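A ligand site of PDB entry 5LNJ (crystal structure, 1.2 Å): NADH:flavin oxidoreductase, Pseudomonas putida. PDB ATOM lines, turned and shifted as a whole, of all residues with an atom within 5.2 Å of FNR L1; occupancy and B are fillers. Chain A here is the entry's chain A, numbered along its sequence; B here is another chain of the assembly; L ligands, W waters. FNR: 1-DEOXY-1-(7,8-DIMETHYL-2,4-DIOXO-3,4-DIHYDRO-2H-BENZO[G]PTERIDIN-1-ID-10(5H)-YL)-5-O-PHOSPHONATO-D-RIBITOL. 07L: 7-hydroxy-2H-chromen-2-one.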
ATOM      1  N   PRO A  21     -18.119 -29.463  -7.064  1.00  0.00           N
ATOM      2  CA  PRO A  21     -16.962 -29.731  -6.221  1.00  0.00           C
ATOM      3  C   PRO A  21     -17.369 -30.571  -4.999  1.00  0.00           C
ATOM      4  O   PRO A  21     -18.586 -30.601  -4.678  1.00  0.00           O
ATOM      5  CB  PRO A  21     -16.506 -28.329  -5.816  1.00  0.00           C
ATOM      6  CG  PRO A  21     -17.790 -27.552  -5.758  1.00  0.00           C
ATOM      7  CD  PRO A  21     -18.637 -28.091  -6.881  1.00  0.00           C
ATOM      8  N   PRO A  22     -16.396 -31.175  -4.333  1.00  0.00           N
ATOM      9  CA  PRO A  22     -16.690 -31.922  -3.120  1.00  0.00           C
ATOM     10  C   PRO A  22     -17.362 -31.023  -2.089  1.00  0.00           C
ATOM     11  O   PRO A  22     -16.900 -29.931  -1.798  1.00  0.00           O
ATOM     12  CB  PRO A  22     -15.299 -32.431  -2.669  1.00  0.00           C
ATOM     13  CG  PRO A  22     -14.310 -31.475  -3.329  1.00  0.00           C
ATOM     14  CD  PRO A  22     -14.953 -31.123  -4.627  1.00  0.00           C
ATOM     15  N   MET A  23     -18.460 -31.531  -1.537  1.00  0.00           N
ATOM     16  CA  MET A  23     -19.207 -30.812  -0.488  1.00  0.00           C
ATOM     17  C   MET A  23     -19.645 -31.807   0.591  1.00  0.00           C
ATOM     18  O   MET A  23     -20.629 -32.549   0.429  1.00  0.00           O
ATOM     19  CB  MET A  23     -20.436 -30.071  -1.034  1.00  0.00           C
ATOM     20  CG  MET A  23     -20.059 -28.830  -1.859  1.00  0.00           C
ATOM     21  SD  MET A  23     -21.492 -27.944  -2.481  1.00  0.00           S
ATOM     22  CE  MET A  23     -22.041 -29.073  -3.722  1.00  0.00           C
ATOM     23  N   CYS A  24     -18.945 -31.775   1.704  1.00  0.00           N
ATOM     24  CA  CYS A  24     -19.311 -32.569   2.887  1.00  0.00           C
ATOM     25  C   CYS A  24     -20.778 -32.442   3.239  1.00  0.00           C
ATOM     26  O   CYS A  24     -21.338 -31.317   3.286  1.00  0.00           O
ATOM     27  CB  CYS A  24     -18.468 -32.129   4.068  1.00  0.00           C
ATOM     28  SG  CYS A  24     -16.754 -32.708   4.069  1.00  0.00           S
ATOM     29  N   GLN A  25     -21.388 -33.578   3.565  1.00  0.00           N
ATOM     30  CA  GLN A  25     -22.771 -33.656   3.973  1.00  0.00           C
ATOM     31  C   GLN A  25     -22.947 -33.937   5.451  1.00  0.00           C
ATOM     32  O   GLN A  25     -24.049 -33.736   5.976  1.00  0.00           O
ATOM     33  CB  GLN A  25     -23.467 -34.741   3.125  1.00  0.00           C
ATOM     34  CG  GLN A  25     -23.465 -34.438   1.643  1.00  0.00           C
ATOM     35  CD  GLN A  25     -24.279 -33.207   1.328  1.00  0.00           C
ATOM     36  OE1 GLN A  25     -25.521 -33.227   1.420  1.00  0.00           O
ATOM     37  NE2 GLN A  25     -23.592 -32.105   0.960  1.00  0.00           N
ATOM     38  N   TYR A  26     -21.921 -34.454   6.107  1.00  0.00           N
ATOM     39  CA  TYR A  26     -21.963 -34.709   7.550  1.00  0.00           C
ATOM     40  C   TYR A  26     -23.060 -35.695   7.939  1.00  0.00           C
ATOM     41  O   TYR A  26     -23.592 -35.614   9.041  1.00  0.00           O
ATOM     42  CB  TYR A  26     -22.061 -33.393   8.343  1.00  0.00           C
ATOM     43  CG  TYR A  26     -21.057 -32.336   7.904  1.00  0.00           C
ATOM     44  CD1 TYR A  26     -19.781 -32.301   8.462  1.00  0.00           C
ATOM     45  CD2 TYR A  26     -21.381 -31.411   6.921  1.00  0.00           C
ATOM     46  CE1 TYR A  26     -18.847 -31.339   8.048  1.00  0.00           C
ATOM     47  CE2 TYR A  26     -20.466 -30.472   6.505  1.00  0.00           C
ATOM     48  CZ  TYR A  26     -19.198 -30.423   7.081  1.00  0.00           C
ATOM     49  OH  TYR A  26     -18.318 -29.460   6.653  1.00  0.00           O
ATOM     50  N   GLU A  55     -17.765 -35.615  -1.839  1.00  0.00           N
ATOM     51  CA  GLU A  55     -17.200 -34.976  -0.655  1.00  0.00           C
ATOM     52  C   GLU A  55     -15.911 -35.602  -0.128  1.00  0.00           C
ATOM     53  O   GLU A  55     -15.685 -36.812  -0.286  1.00  0.00           O
ATOM     54  CB  GLU A  55     -18.236 -35.005   0.478  1.00  0.00           C
ATOM     55  CG  GLU A  55     -18.630 -36.408   0.964  1.00  0.00           C
ATOM     56  CD  GLU A  55     -19.902 -36.370   1.775  1.00  0.00           C
ATOM     57  OE1 GLU A  55     -19.845 -36.048   2.996  1.00  0.00           O
ATOM     58  OE2 GLU A  55     -20.986 -36.588   1.190  1.00  0.00           O
ATOM     59  N   ALA A  56     -15.172 -34.779   0.608  1.00  0.00           N
ATOM     60  CA  ALA A  56     -13.980 -35.208   1.334  1.00  0.00           C
ATOM     61  C   ALA A  56     -14.273 -36.526   2.065  1.00  0.00           C
ATOM     62  O   ALA A  56     -15.094 -36.573   2.998  1.00  0.00           O
ATOM     63  CB  ALA A  56     -13.574 -34.136   2.337  1.00  0.00           C
ATOM     64  N   GLN A  98     -13.067 -37.064  -3.740  1.00  0.00           N
ATOM     65  CA  GLN A  98     -11.976 -36.408  -3.035  1.00  0.00           C
ATOM     66  C   GLN A  98     -11.575 -37.233  -1.817  1.00  0.00           C
ATOM     67  O   GLN A  98     -12.422 -37.465  -0.946  1.00  0.00           O
ATOM     68  CB  GLN A  98     -12.411 -34.996  -2.613  1.00  0.00           C
ATOM     69  CG  GLN A  98     -11.266 -34.199  -2.026  1.00  0.00           C
ATOM     70  CD  GLN A  98     -11.733 -32.917  -1.408  1.00  0.00           C
ATOM     71  OE1 GLN A  98     -12.527 -32.942  -0.484  1.00  0.00           O
ATOM     72  NE2 GLN A  98     -11.216 -31.777  -1.879  1.00  0.00           N
ATOM     73  N   GLU A 175      -9.411 -36.859  -6.595  1.00  0.00           N
ATOM     74  CA  GLU A 175      -8.845 -35.597  -6.134  1.00  0.00           C
ATOM     75  C   GLU A 175      -8.203 -35.773  -4.759  1.00  0.00           C
ATOM     76  O   GLU A 175      -8.886 -36.165  -3.812  1.00  0.00           O
ATOM     77  CB  GLU A 175      -9.921 -34.511  -6.094  1.00  0.00           C
ATOM     78  CG  GLU A 175      -9.346 -33.159  -5.732  1.00  0.00           C
ATOM     79  CD  GLU A 175     -10.405 -32.067  -5.716  1.00  0.00           C
ATOM     80  OE1 GLU A 175     -10.849 -31.647  -6.797  1.00  0.00           O
ATOM     81  OE2 GLU A 175     -10.796 -31.604  -4.643  1.00  0.00           O
ATOM     82  N   HIS A 177      -6.957 -34.289  -1.438  1.00  0.00           N
ATOM     83  CA  HIS A 177      -7.292 -33.069  -0.715  1.00  0.00           C
ATOM     84  C   HIS A 177      -6.089 -32.497   0.019  1.00  0.00           C
ATOM     85  O   HIS A 177      -5.851 -32.810   1.202  1.00  0.00           O
ATOM     86  CB  HIS A 177      -8.422 -33.330   0.285  1.00  0.00           C
ATOM     87  CG  HIS A 177      -9.091 -32.088   0.753  1.00  0.00           C
ATOM     88  ND1 HIS A 177      -8.581 -30.820   0.498  1.00  0.00           N
ATOM     89  CD2 HIS A 177     -10.263 -31.912   1.409  1.00  0.00           C
ATOM     90  CE1 HIS A 177      -9.435 -29.927   0.981  1.00  0.00           C
ATOM     91  NE2 HIS A 177     -10.463 -30.561   1.537  1.00  0.00           N
ATOM     92  N   HIS A 180      -7.248 -26.371   2.352  1.00  0.00           N
ATOM     93  CA  HIS A 180      -8.167 -26.040   3.424  1.00  0.00           C
ATOM     94  C   HIS A 180      -7.634 -26.323   4.832  1.00  0.00           C
ATOM     95  O   HIS A 180      -8.403 -26.541   5.763  1.00  0.00           O
ATOM     96  CB  HIS A 180      -9.550 -26.666   3.156  1.00  0.00           C
ATOM     97  CG  HIS A 180     -10.112 -26.253   1.820  1.00  0.00           C
ATOM     98  ND1 HIS A 180     -11.213 -26.852   1.217  1.00  0.00           N
ATOM     99  CD2 HIS A 180      -9.733 -25.270   0.961  1.00  0.00           C
ATOM    100  CE1 HIS A 180     -11.456 -26.275   0.057  1.00  0.00           C
ATOM    101  NE2 HIS A 180     -10.579 -25.310  -0.121  1.00  0.00           N
ATOM    102  N   ARG A 230      -6.559 -30.820  -4.942  1.00  0.00           N
ATOM    103  CA  ARG A 230      -6.985 -29.497  -4.506  1.00  0.00           C
ATOM    104  C   ARG A 230      -5.890 -28.949  -3.617  1.00  0.00           C
ATOM    105  O   ARG A 230      -5.363 -29.649  -2.731  1.00  0.00           O
ATOM    106  CB  ARG A 230      -8.318 -29.539  -3.739  1.00  0.00           C
ATOM    107  CG  ARG A 230      -8.976 -28.152  -3.678  1.00  0.00           C
ATOM    108  CD  ARG A 230     -10.448 -28.212  -3.242  1.00  0.00           C
ATOM    109  NE  ARG A 230     -11.154 -27.070  -3.829  1.00  0.00           N
ATOM    110  CZ  ARG A 230     -12.454 -26.816  -3.658  1.00  0.00           C
ATOM    111  NH1 ARG A 230     -13.021 -25.828  -4.335  1.00  0.00           N
ATOM    112  NH2 ARG A 230     -13.200 -27.556  -2.827  1.00  0.00           N
ATOM    113  N   ALA A 300     -13.469 -22.278  -7.491  1.00  0.00           N
ATOM    114  CA  ALA A 300     -14.810 -22.146  -6.968  1.00  0.00           C
ATOM    115  C   ALA A 300     -14.815 -20.847  -6.162  1.00  0.00           C
ATOM    116  O   ALA A 300     -14.006 -19.966  -6.433  1.00  0.00           O
ATOM    117  CB  ALA A 300     -15.191 -23.364  -6.096  1.00  0.00           C
ATOM    118  N   TRP A 301     -15.708 -20.762  -5.172  1.00  0.00           N
ATOM    119  CA  TRP A 301     -15.819 -19.616  -4.269  1.00  0.00           C
ATOM    120  C   TRP A 301     -16.343 -18.375  -4.948  1.00  0.00           C
ATOM    121  O   TRP A 301     -15.737 -17.296  -4.850  1.00  0.00           O
ATOM    122  CB  TRP A 301     -14.502 -19.314  -3.581  1.00  0.00           C
ATOM    123  CG  TRP A 301     -13.883 -20.486  -2.913  1.00  0.00           C
ATOM    124  CD1 TRP A 301     -12.792 -21.183  -3.343  1.00  0.00           C
ATOM    125  CD2 TRP A 301     -14.275 -21.082  -1.676  1.00  0.00           C
ATOM    126  NE1 TRP A 301     -12.509 -22.193  -2.467  1.00  0.00           N
ATOM    127  CE2 TRP A 301     -13.403 -22.149  -1.435  1.00  0.00           C
ATOM    128  CE3 TRP A 301     -15.303 -20.835  -0.766  1.00  0.00           C
ATOM    129  CZ2 TRP A 301     -13.522 -22.974  -0.317  1.00  0.00           C
ATOM    130  CZ3 TRP A 301     -15.415 -21.640   0.346  1.00  0.00           C
ATOM    131  CH2 TRP A 301     -14.528 -22.692   0.560  1.00  0.00           C
ATOM    132  N   GLY A 302     -17.488 -18.499  -5.624  1.00  0.00           N
ATOM    133  CA  GLY A 302     -18.136 -17.355  -6.228  1.00  0.00           C
ATOM    134  C   GLY A 302     -18.316 -17.402  -7.738  1.00  0.00           C
ATOM    135  O   GLY A 302     -18.596 -16.341  -8.294  1.00  0.00           O
ATOM    136  N   PHE A 303     -18.185 -18.532  -8.428  1.00  0.00           N
ATOM    137  CA  PHE A 303     -18.474 -18.615  -9.873  1.00  0.00           C
ATOM    138  C   PHE A 303     -19.896 -19.095 -10.196  1.00  0.00           C
ATOM    139  O   PHE A 303     -20.202 -19.322 -11.348  1.00  0.00           O
ATOM    140  CB  PHE A 303     -17.490 -19.532 -10.585  1.00  0.00           C
ATOM    141  CG  PHE A 303     -16.080 -19.057 -10.551  1.00  0.00           C
ATOM    142  CD1 PHE A 303     -15.606 -18.173 -11.511  1.00  0.00           C
ATOM    143  CD2 PHE A 303     -15.195 -19.511  -9.590  1.00  0.00           C
ATOM    144  CE1 PHE A 303     -14.295 -17.750 -11.481  1.00  0.00           C
ATOM    145  CE2 PHE A 303     -13.895 -19.080  -9.562  1.00  0.00           C
ATOM    146  CZ  PHE A 303     -13.439 -18.204 -10.507  1.00  0.00           C
ATOM    147  N   GLY A 304     -20.755 -19.168  -9.189  1.00  0.00           N
ATOM    148  CA  GLY A 304     -22.072 -19.779  -9.344  1.00  0.00           C
ATOM    149  C   GLY A 304     -23.191 -18.930  -9.922  1.00  0.00           C
ATOM    150  O   GLY A 304     -24.322 -18.911  -9.406  1.00  0.00           O
ATOM    151  N   SER A 322     -16.234 -24.902 -11.078  1.00  0.00           N
ATOM    152  CA  SER A 322     -16.848 -25.603  -9.951  1.00  0.00           C
ATOM    153  C   SER A 322     -17.936 -24.736  -9.348  1.00  0.00           C
ATOM    154  O   SER A 322     -17.683 -23.579  -8.997  1.00  0.00           O
ATOM    155  CB  SER A 322     -15.790 -25.961  -8.935  1.00  0.00           C
ATOM    156  OG  SER A 322     -14.869 -26.925  -9.480  1.00  0.00           O
ATOM    157  N   VAL A 323     -19.132 -25.311  -9.215  1.00  0.00           N
ATOM    158  CA  VAL A 323     -20.315 -24.608  -8.722  1.00  0.00           C
ATOM    159  C   VAL A 323     -20.904 -25.455  -7.570  1.00  0.00           C
ATOM    160  O   VAL A 323     -21.457 -26.538  -7.788  1.00  0.00           O
ATOM    161  CB  VAL A 323     -21.328 -24.411  -9.858  1.00  0.00           C
ATOM    162  CG1 VAL A 323     -22.613 -23.746  -9.310  1.00  0.00           C
ATOM    163  CG2 VAL A 323     -20.713 -23.583 -10.977  1.00  0.00           C
ATOM    164  N   GLY A 324     -20.739 -24.955  -6.349  1.00  0.00           N
ATOM    165  CA  GLY A 324     -21.083 -25.696  -5.131  1.00  0.00           C
ATOM    166  C   GLY A 324     -22.451 -25.353  -4.547  1.00  0.00           C
ATOM    167  O   GLY A 324     -23.446 -26.072  -4.777  1.00  0.00           O
ATOM    168  N   ARG A 325     -22.533 -24.248  -3.815  1.00  0.00           N
ATOM    169  CA  ARG A 325     -23.758 -23.905  -3.093  1.00  0.00           C
ATOM    170  C   ARG A 325     -24.958 -23.754  -4.003  1.00  0.00           C
ATOM    171  O   ARG A 325     -26.069 -24.116  -3.605  1.00  0.00           O
ATOM    172  CB  ARG A 325     -23.548 -22.664  -2.236  1.00  0.00           C
ATOM    173  CG  ARG A 325     -22.751 -23.000  -0.983  1.00  0.00           C
ATOM    174  CD  ARG A 325     -22.265 -21.783  -0.260  1.00  0.00           C
ATOM    175  NE  ARG A 325     -21.231 -21.145  -1.047  1.00  0.00           N
ATOM    176  CZ  ARG A 325     -20.585 -20.051  -0.666  1.00  0.00           C
ATOM    177  NH1 ARG A 325     -20.904 -19.458   0.477  1.00  0.00           N
ATOM    178  NH2 ARG A 325     -19.644 -19.528  -1.452  1.00  0.00           N
ATOM    179  N   ALA A 326     -24.768 -23.245  -5.211  1.00  0.00           N
ATOM    180  CA  ALA A 326     -25.915 -23.119  -6.122  1.00  0.00           C
ATOM    181  C   ALA A 326     -26.570 -24.483  -6.417  1.00  0.00           C
ATOM    182  O   ALA A 326     -27.784 -24.533  -6.697  1.00  0.00           O
ATOM    183  CB  ALA A 326     -25.495 -22.439  -7.405  1.00  0.00           C
ATOM    184  N   LEU A 328     -26.658 -26.982  -4.116  1.00  0.00           N
ATOM    185  CA  LEU A 328     -27.452 -27.302  -2.924  1.00  0.00           C
ATOM    186  C   LEU A 328     -28.810 -26.597  -2.994  1.00  0.00           C
ATOM    187  O   LEU A 328     -29.842 -27.183  -2.650  1.00  0.00           O
ATOM    188  CB  LEU A 328     -26.706 -26.893  -1.659  1.00  0.00           C
ATOM    189  CG  LEU A 328     -25.291 -27.449  -1.480  1.00  0.00           C
ATOM    190  CD1 LEU A 328     -24.692 -26.986  -0.148  1.00  0.00           C
ATOM    191  CD2 LEU A 328     -25.244 -28.967  -1.626  1.00  0.00           C
ATOM    192  N   PRO B 353     -28.037 -30.339   5.948  1.00  0.00           N
ATOM    193  CA  PRO B 353     -26.825 -30.319   5.108  1.00  0.00           C
ATOM    194  C   PRO B 353     -26.904 -29.384   3.934  1.00  0.00           C
ATOM    195  O   PRO B 353     -25.870 -29.108   3.318  1.00  0.00           O
ATOM    196  CB  PRO B 353     -26.720 -31.770   4.634  1.00  0.00           C
ATOM    197  CG  PRO B 353     -27.476 -32.579   5.641  1.00  0.00           C
ATOM    198  CD  PRO B 353     -28.613 -31.693   6.058  1.00  0.00           C
ATOM    199  N   TRP B 357     -25.891 -23.883   4.894  1.00  0.00           N
ATOM    200  CA  TRP B 357     -25.008 -23.156   3.955  1.00  0.00           C
ATOM    201  C   TRP B 357     -25.718 -22.099   3.163  1.00  0.00           C
ATOM    202  O   TRP B 357     -25.078 -21.250   2.557  1.00  0.00           O
ATOM    203  CB  TRP B 357     -24.354 -24.167   3.019  1.00  0.00           C
ATOM    204  CG  TRP B 357     -23.705 -25.255   3.796  1.00  0.00           C
ATOM    205  CD1 TRP B 357     -24.179 -26.514   3.950  1.00  0.00           C
ATOM    206  CD2 TRP B 357     -22.557 -25.132   4.628  1.00  0.00           C
ATOM    207  NE1 TRP B 357     -23.364 -27.210   4.808  1.00  0.00           N
ATOM    208  CE2 TRP B 357     -22.348 -26.400   5.219  1.00  0.00           C
ATOM    209  CE3 TRP B 357     -21.667 -24.099   4.911  1.00  0.00           C
ATOM    210  CZ2 TRP B 357     -21.292 -26.646   6.069  1.00  0.00           C
ATOM    211  CZ3 TRP B 357     -20.621 -24.357   5.756  1.00  0.00           C
ATOM    212  CH2 TRP B 357     -20.426 -25.634   6.319  1.00  0.00           C
HETATM  213  C9A FNR L   1     -17.593 -27.351   1.003  1.00  0.00           C
HETATM  214  N10 FNR L   1     -16.274 -27.232   0.456  1.00  0.00           N
HETATM  215  CAA FNR L   1     -15.448 -28.371   0.483  1.00  0.00           C
HETATM  216  N1  FNR L   1     -14.261 -28.302  -0.158  1.00  0.00           N
HETATM  217  C2  FNR L   1     -13.510 -29.437  -0.290  1.00  0.00           C
HETATM  218  O2  FNR L   1     -12.381 -29.387  -0.856  1.00  0.00           O
HETATM  219  N3  FNR L   1     -13.959 -30.618   0.278  1.00  0.00           N
HETATM  220  C4  FNR L   1     -15.206 -30.748   0.829  1.00  0.00           C
HETATM  221  O4  FNR L   1     -15.661 -31.878   1.112  1.00  0.00           O
HETATM  222  C4A FNR L   1     -15.877 -29.539   1.128  1.00  0.00           C
HETATM  223  N5  FNR L   1     -17.069 -29.541   1.909  1.00  0.00           N
HETATM  224  C5A FNR L   1     -17.974 -28.486   1.716  1.00  0.00           C
HETATM  225  C6  FNR L   1     -19.315 -28.606   2.183  1.00  0.00           C
HETATM  226  C7  FNR L   1     -20.263 -27.619   1.868  1.00  0.00           C
HETATM  227  C7M FNR L   1     -21.668 -27.883   2.246  1.00  0.00           C
HETATM  228  C8  FNR L   1     -19.842 -26.433   1.250  1.00  0.00           C
HETATM  229  C8M FNR L   1     -20.838 -25.359   0.929  1.00  0.00           C
HETATM  230  C9  FNR L   1     -18.512 -26.271   0.868  1.00  0.00           C
HETATM  231  C1' FNR L   1     -15.935 -26.117  -0.476  1.00  0.00           C
HETATM  232  C2' FNR L   1     -16.660 -26.263  -1.816  1.00  0.00           C
HETATM  233  O2' FNR L   1     -16.092 -27.328  -2.601  1.00  0.00           O
HETATM  234  C3' FNR L   1     -16.571 -24.970  -2.640  1.00  0.00           C
HETATM  235  O3' FNR L   1     -15.194 -24.603  -2.812  1.00  0.00           O
HETATM  236  C4' FNR L   1     -17.310 -23.795  -1.998  1.00  0.00           C
HETATM  237  O4' FNR L   1     -18.667 -24.187  -1.769  1.00  0.00           O
HETATM  238  C5' FNR L   1     -17.225 -22.535  -2.865  1.00  0.00           C
HETATM  239  O5' FNR L   1     -17.926 -22.685  -4.112  1.00  0.00           O
HETATM  240  P   FNR L   1     -19.411 -22.015  -4.303  1.00  0.00           P
HETATM  241  O1P FNR L   1     -20.261 -22.629  -3.222  1.00  0.00           O
HETATM  242  O2P FNR L   1     -19.245 -20.532  -4.102  1.00  0.00           O
HETATM  243  O3P FNR L   1     -19.840 -22.419  -5.683  1.00  0.00           O
HETATM  244  O11 07L L   2     -12.587 -28.896   2.577  1.00  0.00           O
HETATM  245  C9  07L L   2     -13.576 -28.656   3.203  1.00  0.00           C
HETATM  246  C8  07L L   2     -14.438 -29.407   3.999  1.00  0.00           C
HETATM  247  C7  07L L   2     -15.567 -28.852   4.578  1.00  0.00           C
HETATM  248  C2  07L L   2     -15.864 -27.519   4.315  1.00  0.00           C
HETATM  249  O10 07L L   2     -13.864 -27.317   3.000  1.00  0.00           O
HETATM  250  C3  07L L   2     -15.001 -26.753   3.536  1.00  0.00           C
HETATM  251  C4  07L L   2     -15.225 -25.428   3.213  1.00  0.00           C
HETATM  252  C5  07L L   2     -16.331 -24.784   3.723  1.00  0.00           C
HETATM  253  O12 07L L   2     -16.587 -23.470   3.450  1.00  0.00           O
HETATM  254  C6  07L L   2     -17.216 -25.508   4.515  1.00  0.00           C
HETATM  255  C1  07L L   2     -16.984 -26.850   4.809  1.00  0.00           C
HETATM  256  O   HOH W   1     -18.210 -21.286  -7.538  1.00  0.00           O
HETATM  257  O   HOH W   2     -22.548 -21.800  -6.151  1.00  0.00           O
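Pro 21 touches FNR L1 (CB to O2', 3.4 Å).
Met 23 touches FNR L1 (CA to C5A, 3.4 Å).
Glu 55 touches FNR L1.
CB of Ala 300 touches O5' of FNR L1, at 3.4 Å.
Val 323 touches FNR L1 (C to O3P, 3.7 Å).
CD1 of Leu 328 touches C7M of FNR L1, at 3.96 Å.
NE1 of Trp 357 of chain B touches C7M of FNR L1 (3.1 Å).
18 residues have an atom within 4 Å of FNR L1: Pro 21, Pro 22, Met 23, Cys 24, Glu 55, Ala 56, Gln 98, His 177, His 180, Arg 230, Ala 300, Trp 301, Gly 302, Val 323, Gly 324, Arg 325, Leu 328 and Trp 357 of chain B.
Water W2 lies within hydrogen-bond range of N of Ala 326 (2.8 Å), O3P of FNR L1 (2.8 Å) and N of Arg 325 (3.4 Å).
OE1 of Gln 98 sits at hydrogen-bond distance from N3 of FNR L1, at 2.8 Å.
A ring nitrogen (NE2) of His 177 is in hydrogen-bond range of an oxygen (O2) of FNR L1.
An oxygen (O3P) of FNR L1 is in hydrogen-bond range of the backbone NH (N) of Gly 324 (2.8 Å).
NE of Arg 325 lies within salt-bridge range of O1P of FNR L1 (2.8 Å).
The backbone NH (N) of Trp 301 is in hydrogen-bond range of an oxygen (O5') of FNR L1 (3.1 Å).
An oxygen (O2') of FNR L1 lies within hydrogen-bond range of the backbone carbonyl oxygen (O) of Pro 22 (2.8 Å).
A ring nitrogen (NE2) of His 177 lies within hydrogen-bond range of an oxygen (O11) of 07L L2, 2.9 Å away.
The side-chain sulfur of Cys 24 lies within hydrogen-bond range of an oxygen (O4) of FNR L1 (3.3 Å).
An oxygen (O11) of 07L L2 lies within hydrogen-bond range of a ring nitrogen (ND1) of His 180, at 2.8 Å.
N of Gly 302 is in hydrogen-bond range of O2P of FNR L1.
ND1 of His 180 sits close to O2 of FNR L1 (3.5 Å).
NH2 of Arg 230 is in hydrogen-bond range of O2 of FNR L1 (2.8 Å).
The backbone NH (N) of Ala 56 sits at hydrogen-bond distance from an oxygen (O4) of FNR L1, at 3.0 Å.
The backbone NH (N) of Cys 24 sits close to an oxygen (O4) of FNR L1 (3.3 Å).
The backbone NH (N) of Arg 325 is in hydrogen-bond range of an oxygen (O1P) of FNR L1, 2.9 Å away.
The side-chain carboxylate (OE1) of Glu 55 sits at hydrogen-bond distance from the backbone NH (N) of Gln 25 (3.0 Å).
NE2 of Gln 98 sits at hydrogen-bond distance from OE2 of Glu 175 (2.8 Å).
The indole nitrogen of Trp 357 of chain B sits close to the backbone carbonyl oxygen of Pro 353 of chain B (3.5 Å).
The backbone NH of Ala 56 lies close to the side-chain amide oxygen of Gln 98, at 3.4 Å.
The backbone carbonyl oxygen (O) of Met 23 sits at hydrogen-bond distance from the side-chain amide nitrogen (NE2) of Gln 25 (3.0 Å).
A nitrogen (N3) of FNR L1 sits close to an oxygen (O11) of 07L L2 (3.2 Å).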
